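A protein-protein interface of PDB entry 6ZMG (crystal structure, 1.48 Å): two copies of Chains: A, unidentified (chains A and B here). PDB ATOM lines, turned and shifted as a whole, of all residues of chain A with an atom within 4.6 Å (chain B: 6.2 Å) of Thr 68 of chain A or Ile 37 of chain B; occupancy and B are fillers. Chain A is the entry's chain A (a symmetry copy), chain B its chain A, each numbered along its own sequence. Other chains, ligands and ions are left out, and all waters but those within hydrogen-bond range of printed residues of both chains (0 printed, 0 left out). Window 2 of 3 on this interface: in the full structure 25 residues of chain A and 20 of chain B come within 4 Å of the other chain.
O of Arg 55 of chain A is in hydrogen-bond range of N of Phe 51 of chain B, 2.8 Å away.
OE2 of Glu 30 of chain B lies within salt-bridge range of NH2 of Arg 55 of chain A.
NH1 of Arg 40 of chain B is in hydrogen-bond range of O of Pro 47 of chain B (3.0 Å).
Val 33 of chain B touches Val 57 of chain A.
Val 57 of chain A touches Ile 37 of chain B.
CG2 of Val 57 of chain A touches CE1 of Phe 51 of chain B, 3.7 Å away.
Leu 66 of chain A touches Ile 37 of chain B.
Lys 41 of chain B touches Leu 66 of chain A (CE to CD2, 3.6 Å).
Leu 66 of chain A touches Pro 47 of chain B (CD1 to CG, 3.5 Å).
OE2 of Glu 30 of chain B touches CG2 of Thr 68 of chain A (3.8 Å).
Ile 37 of chain B touches Thr 68 of chain A (CD1 to OG1, 3.8 Å).
Printed residues of chain B within 4 Å of Arg 55 of chain A: Glu 30 and Phe 51.
Printed residues of chain B within 4 Å of Val 57 of chain A: Val 33 (3.9 Å), Ile 37 (3.8 Å) and Phe 51 (3.7 Å).
Of the printed residues of chain B, Thr 68 of chain A touches Glu 30 and Ile 37.
Of the printed residues of chain A, Lys 41 of chain B touches Leu 66 (3.6 Å).
Of the printed residues of chain A, Pro 47 of chain B touches Leu 66 (3.5 Å).
The nearest printed residue of chain B that does not touch Thr 68 of chain A is Val 33 of chain B (4.02 Å).
Of the 14 printed residues of chain B, 6 touch a printed residue of chain A.
Hydrophobic or aromatic side chains of chain B within 4 Å of the printed part of chain A: Val 33, Ile 37, Pro 47 and Phe 51.
Hydrophobic or aromatic side chains of chain A within 4 Å of the printed part of chain B: Val 57 and Leu 66.
Among the printed residues, 10 pairs touch across the chains.
No position is printed for both chains.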
ATOM      1  N   ASN A  20      -4.384  20.321  22.662  1.00  0.00           N
ATOM      2  CA  ASN A  20      -3.464  20.054  23.751  1.00  0.00           C
ATOM      3  C   ASN A  20      -2.043  19.996  23.209  1.00  0.00           C
ATOM      4  O   ASN A  20      -1.805  19.493  22.107  1.00  0.00           O
ATOM      5  CB  ASN A  20      -3.719  18.678  24.368  1.00  0.00           C
ATOM      6  CG  ASN A  20      -4.699  18.692  25.518  1.00  0.00           C
ATOM      7  OD1 ASN A  20      -5.516  19.591  25.675  1.00  0.00           O
ATOM      8  ND2 ASN A  20      -4.623  17.654  26.332  1.00  0.00           N
ATOM      9  N   ARG A  55     -14.384  17.360  20.810  1.00  0.00           N
ATOM     10  CA  ARG A  55     -13.592  16.704  21.834  1.00  0.00           C
ATOM     11  C   ARG A  55     -12.915  15.510  21.176  1.00  0.00           C
ATOM     12  O   ARG A  55     -13.541  14.770  20.415  1.00  0.00           O
ATOM     13  CB  ARG A  55     -14.458  16.256  23.009  1.00  0.00           C
ATOM     14  CG  ARG A  55     -15.087  17.408  23.773  1.00  0.00           C
ATOM     15  CD  ARG A  55     -14.076  18.219  24.541  1.00  0.00           C
ATOM     16  NE  ARG A  55     -13.671  17.531  25.751  1.00  0.00           N
ATOM     17  CZ  ARG A  55     -12.592  17.833  26.459  1.00  0.00           C
ATOM     18  NH1 ARG A  55     -11.767  18.805  26.070  1.00  0.00           N
ATOM     19  NH2 ARG A  55     -12.343  17.149  27.559  1.00  0.00           N
ATOM     20  N   GLY A  56     -11.636  15.332  21.457  1.00  0.00           N
ATOM     21  CA  GLY A  56     -10.865  14.262  20.869  1.00  0.00           C
ATOM     22  C   GLY A  56     -10.262  13.409  21.961  1.00  0.00           C
ATOM     23  O   GLY A  56      -9.873  13.911  23.017  1.00  0.00           O
ATOM     24  N   VAL A  57     -10.161  12.114  21.681  1.00  0.00           N
ATOM     25  CA  VAL A  57      -9.466  11.158  22.527  1.00  0.00           C
ATOM     26  C   VAL A  57      -8.333  10.574  21.708  1.00  0.00           C
ATOM     27  O   VAL A  57      -8.546  10.142  20.569  1.00  0.00           O
ATOM     28  CB  VAL A  57     -10.429  10.054  22.985  1.00  0.00           C
ATOM     29  CG1 VAL A  57      -9.664   8.998  23.761  1.00  0.00           C
ATOM     30  CG2 VAL A  57     -11.525  10.666  23.805  1.00  0.00           C
ATOM     31  N   LEU A  66      -3.509   8.012  27.595  1.00  0.00           N
ATOM     32  CA  LEU A  66      -4.740   8.373  26.917  1.00  0.00           C
ATOM     33  C   LEU A  66      -5.119   9.778  27.346  1.00  0.00           C
ATOM     34  O   LEU A  66      -5.272  10.045  28.544  1.00  0.00           O
ATOM     35  CB  LEU A  66      -5.855   7.424  27.324  1.00  0.00           C
ATOM     36  CG  LEU A  66      -7.121   7.592  26.491  1.00  0.00           C
ATOM     37  CD1 LEU A  66      -6.875   7.114  25.074  1.00  0.00           C
ATOM     38  CD2 LEU A  66      -8.226   6.818  27.161  1.00  0.00           C
ATOM     39  N   VAL A  67      -5.292  10.656  26.372  1.00  0.00           N
ATOM     40  CA  VAL A  67      -5.580  12.053  26.624  1.00  0.00           C
ATOM     41  C   VAL A  67      -6.890  12.429  25.953  1.00  0.00           C
ATOM     42  O   VAL A  67      -7.204  11.954  24.856  1.00  0.00           O
ATOM     43  CB  VAL A  67      -4.447  12.950  26.080  1.00  0.00           C
ATOM     44  CG1 VAL A  67      -4.715  14.393  26.459  1.00  0.00           C
ATOM     45  CG2 VAL A  67      -3.078  12.482  26.574  1.00  0.00           C
ATOM     46  N   THR A  68      -7.642  13.301  26.612  1.00  0.00           N
ATOM     47  CA  THR A  68      -8.836  13.914  26.052  1.00  0.00           C
ATOM     48  C   THR A  68      -8.538  15.397  25.906  1.00  0.00           C
ATOM     49  O   THR A  68      -8.023  16.019  26.839  1.00  0.00           O
ATOM     50  CB  THR A  68     -10.032  13.687  26.971  1.00  0.00           C
ATOM     51  OG1 THR A  68     -10.189  12.280  27.178  1.00  0.00           O
ATOM     52  CG2 THR A  68     -11.314  14.221  26.363  1.00  0.00           C
ATOM     53  N   GLU A  69      -8.820  15.948  24.728  1.00  0.00           N
ATOM     54  CA  GLU A  69      -8.494  17.329  24.430  1.00  0.00           C
ATOM     55  C   GLU A  69      -9.633  17.954  23.644  1.00  0.00           C
ATOM     56  O   GLU A  69     -10.524  17.267  23.142  1.00  0.00           O
ATOM     57  CB  GLU A  69      -7.218  17.429  23.573  1.00  0.00           C
ATOM     58  CG  GLU A  69      -7.326  16.684  22.246  1.00  0.00           C
ATOM     59  CD  GLU A  69      -6.066  16.756  21.383  1.00  0.00           C
ATOM     60  OE1 GLU A  69      -5.081  17.428  21.771  1.00  0.00           O
ATOM     61  OE2 GLU A  69      -6.052  16.099  20.313  1.00  0.00           O
ATOM     62  N   GLU B  30     -19.567  15.376  27.241  1.00  0.00           N
ATOM     63  CA  GLU B  30     -18.498  14.749  28.014  1.00  0.00           C
ATOM     64  C   GLU B  30     -18.931  13.420  28.617  1.00  0.00           C
ATOM     65  O   GLU B  30     -18.100  12.518  28.767  1.00  0.00           O
ATOM     66  CB  GLU B  30     -17.920  15.669  29.077  1.00  0.00           C
ATOM     67  CG  GLU B  30     -16.435  15.295  29.433  1.00  0.00           C
ATOM     68  CD  GLU B  30     -15.388  15.570  28.322  1.00  0.00           C
ATOM     69  OE1 GLU B  30     -15.718  16.153  27.253  1.00  0.00           O
ATOM     70  OE2 GLU B  30     -14.206  15.194  28.544  1.00  0.00           O
ATOM     71  N   VAL B  32     -20.782  11.266  27.082  1.00  0.00           N
ATOM     72  CA  VAL B  32     -20.611  10.331  25.974  1.00  0.00           C
ATOM     73  C   VAL B  32     -19.134  10.019  25.745  1.00  0.00           C
ATOM     74  O   VAL B  32     -18.775   8.860  25.505  1.00  0.00           O
ATOM     75  CB  VAL B  32     -21.309  10.868  24.714  1.00  0.00           C
ATOM     76  CG1 VAL B  32     -21.009   9.968  23.501  1.00  0.00           C
ATOM     77  CG2 VAL B  32     -22.815  10.935  24.951  1.00  0.00           C
ATOM     78  N   VAL B  33     -18.262  11.036  25.822  1.00  0.00           N
ATOM     79  CA  VAL B  33     -16.820  10.807  25.697  1.00  0.00           C
ATOM     80  C   VAL B  33     -16.362   9.787  26.736  1.00  0.00           C
ATOM     81  O   VAL B  33     -15.692   8.797  26.416  1.00  0.00           O
ATOM     82  CB  VAL B  33     -16.054  12.138  25.851  1.00  0.00           C
ATOM     83  CG1 VAL B  33     -14.568  11.914  25.901  1.00  0.00           C
ATOM     84  CG2 VAL B  33     -16.371  13.129  24.743  1.00  0.00           C
ATOM     85  N   LYS B  34     -16.697  10.034  28.004  1.00  0.00           N
ATOM     86  CA  LYS B  34     -16.215   9.165  29.070  1.00  0.00           C
ATOM     87  C   LYS B  34     -16.778   7.758  28.941  1.00  0.00           C
ATOM     88  O   LYS B  34     -16.063   6.777  29.161  1.00  0.00           O
ATOM     89  CB  LYS B  34     -16.572   9.765  30.426  1.00  0.00           C
ATOM     90  CG  LYS B  34     -15.826  11.032  30.773  1.00  0.00           C
ATOM     91  CD  LYS B  34     -16.327  11.551  32.118  1.00  0.00           C
ATOM     92  CE  LYS B  34     -15.766  12.905  32.407  1.00  0.00           C
ATOM     93  NZ  LYS B  34     -14.331  12.773  32.643  1.00  0.00           N
ATOM     94  N   ASP B  35     -18.055   7.633  28.600  1.00  0.00           N
ATOM     95  CA  ASP B  35     -18.639   6.303  28.485  1.00  0.00           C
ATOM     96  C   ASP B  35     -18.034   5.551  27.312  1.00  0.00           C
ATOM     97  O   ASP B  35     -17.784   4.342  27.408  1.00  0.00           O
ATOM     98  CB  ASP B  35     -20.158   6.402  28.373  1.00  0.00           C
ATOM     99  CG  ASP B  35     -20.859   5.103  28.722  1.00  0.00           C
ATOM    100  OD1 ASP B  35     -20.522   4.490  29.762  1.00  0.00           O
ATOM    101  OD2 ASP B  35     -21.766   4.705  27.952  1.00  0.00           O
ATOM    102  N   THR B  36     -17.789   6.258  26.202  1.00  0.00           N
ATOM    103  CA  THR B  36     -17.192   5.626  25.036  1.00  0.00           C
ATOM    104  C   THR B  36     -15.801   5.121  25.365  1.00  0.00           C
ATOM    105  O   THR B  36     -15.449   4.000  24.995  1.00  0.00           O
ATOM    106  CB  THR B  36     -17.172   6.591  23.850  1.00  0.00           C
ATOM    107  OG1 THR B  36     -18.513   6.946  23.493  1.00  0.00           O
ATOM    108  CG2 THR B  36     -16.489   5.960  22.640  1.00  0.00           C
ATOM    109  N   ILE B  37     -14.999   5.929  26.069  1.00  0.00           N
ATOM    110  CA  ILE B  37     -13.666   5.483  26.463  1.00  0.00           C
ATOM    111  C   ILE B  37     -13.772   4.204  27.266  1.00  0.00           C
ATOM    112  O   ILE B  37     -13.027   3.246  27.036  1.00  0.00           O
ATOM    113  CB  ILE B  37     -12.926   6.567  27.266  1.00  0.00           C
ATOM    114  CG1 ILE B  37     -12.545   7.748  26.380  1.00  0.00           C
ATOM    115  CG2 ILE B  37     -11.670   5.967  27.956  1.00  0.00           C
ATOM    116  CD1 ILE B  37     -12.113   8.953  27.160  1.00  0.00           C
ATOM    117  N   ALA B  38     -14.701   4.182  28.233  1.00  0.00           N
ATOM    118  CA  ALA B  38     -14.826   3.040  29.130  1.00  0.00           C
ATOM    119  C   ALA B  38     -15.223   1.784  28.370  1.00  0.00           C
ATOM    120  O   ALA B  38     -14.659   0.708  28.597  1.00  0.00           O
ATOM    121  CB  ALA B  38     -15.825   3.375  30.235  1.00  0.00           C
ATOM    122  N   ILE B  39     -16.171   1.911  27.444  1.00  0.00           N
ATOM    123  CA  ILE B  39     -16.627   0.766  26.664  1.00  0.00           C
ATOM    124  C   ILE B  39     -15.497   0.235  25.800  1.00  0.00           C
ATOM    125  O   ILE B  39     -15.264  -0.978  25.728  1.00  0.00           O
ATOM    126  CB  ILE B  39     -17.846   1.166  25.813  1.00  0.00           C
ATOM    127  CG1 ILE B  39     -19.051   1.440  26.723  1.00  0.00           C
ATOM    128  CG2 ILE B  39     -18.191   0.081  24.837  1.00  0.00           C
ATOM    129  CD1 ILE B  39     -20.168   2.211  26.080  1.00  0.00           C
ATOM    130  N   ARG B  40     -14.812   1.131  25.095  1.00  0.00           N
ATOM    131  CA  ARG B  40     -13.796   0.710  24.140  1.00  0.00           C
ATOM    132  C   ARG B  40     -12.605   0.110  24.863  1.00  0.00           C
ATOM    133  O   ARG B  40     -12.023  -0.870  24.390  1.00  0.00           O
ATOM    134  CB  ARG B  40     -13.421   1.875  23.218  1.00  0.00           C
ATOM    135  CG  ARG B  40     -14.639   2.444  22.469  1.00  0.00           C
ATOM    136  CD  ARG B  40     -14.256   3.305  21.295  1.00  0.00           C
ATOM    137  NE  ARG B  40     -13.962   2.468  20.141  1.00  0.00           N
ATOM    138  CZ  ARG B  40     -13.200   2.836  19.120  1.00  0.00           C
ATOM    139  NH1 ARG B  40     -12.600   4.022  19.114  1.00  0.00           N
ATOM    140  NH2 ARG B  40     -13.034   2.006  18.105  1.00  0.00           N
ATOM    141  N   LYS B  41     -12.259   0.636  26.039  1.00  0.00           N
ATOM    142  CA  LYS B  41     -11.215  -0.009  26.826  1.00  0.00           C
ATOM    143  C   LYS B  41     -11.585  -1.455  27.164  1.00  0.00           C
ATOM    144  O   LYS B  41     -10.730  -2.352  27.105  1.00  0.00           O
ATOM    145  CB  LYS B  41     -10.941   0.786  28.096  1.00  0.00           C
ATOM    146  CG  LYS B  41     -10.138   2.036  27.875  1.00  0.00           C
ATOM    147  CD  LYS B  41     -10.044   2.812  29.178  1.00  0.00           C
ATOM    148  CE  LYS B  41      -9.041   3.946  29.122  1.00  0.00           C
ATOM    149  NZ  LYS B  41      -8.937   4.599  30.473  1.00  0.00           N
ATOM    150  N   ARG B  42     -12.859  -1.711  27.505  1.00  0.00           N
ATOM    151  CA  ARG B  42     -13.252  -3.081  27.838  1.00  0.00           C
ATOM    152  C   ARG B  42     -13.268  -3.991  26.617  1.00  0.00           C
ATOM    153  O   ARG B  42     -13.169  -5.218  26.762  1.00  0.00           O
ATOM    154  CB  ARG B  42     -14.593  -3.130  28.554  1.00  0.00           C
ATOM    155  CG  ARG B  42     -14.552  -2.531  29.948  1.00  0.00           C
ATOM    156  CD  ARG B  42     -15.865  -2.781  30.711  1.00  0.00           C
ATOM    157  NE  ARG B  42     -17.005  -2.086  30.108  1.00  0.00           N
ATOM    158  CZ  ARG B  42     -17.440  -0.875  30.468  1.00  0.00           C
ATOM    159  NH1 ARG B  42     -16.837  -0.199  31.443  1.00  0.00           N
ATOM    160  NH2 ARG B  42     -18.490  -0.341  29.858  1.00  0.00           N
ATOM    161  N   PRO B  47      -9.116   3.431  21.973  1.00  0.00           N
ATOM    162  CA  PRO B  47     -10.357   4.213  22.078  1.00  0.00           C
ATOM    163  C   PRO B  47     -10.404   5.447  21.209  1.00  0.00           C
ATOM    164  O   PRO B  47     -11.481   6.043  21.076  1.00  0.00           O
ATOM    165  CB  PRO B  47     -10.404   4.625  23.553  1.00  0.00           C
ATOM    166  CG  PRO B  47      -9.041   4.548  24.010  1.00  0.00           C
ATOM    167  CD  PRO B  47      -8.344   3.471  23.224  1.00  0.00           C
ATOM    168  N   PHE B  51     -15.407  13.499  18.835  1.00  0.00           N
ATOM    169  CA  PHE B  51     -16.769  13.681  19.317  1.00  0.00           C
ATOM    170  C   PHE B  51     -17.213  15.096  18.978  1.00  0.00           C
ATOM    171  O   PHE B  51     -16.594  16.066  19.419  1.00  0.00           O
ATOM    172  CB  PHE B  51     -16.842  13.453  20.828  1.00  0.00           C
ATOM    173  CG  PHE B  51     -16.357  12.098  21.268  1.00  0.00           C
ATOM    174  CD1 PHE B  51     -15.005  11.813  21.370  1.00  0.00           C
ATOM    175  CD2 PHE B  51     -17.258  11.121  21.581  1.00  0.00           C
ATOM    176  CE1 PHE B  51     -14.582  10.562  21.772  1.00  0.00           C
ATOM    177  CE2 PHE B  51     -16.854   9.890  21.994  1.00  0.00           C
ATOM    178  CZ  PHE B  51     -15.513   9.609  22.103  1.00  0.00           C
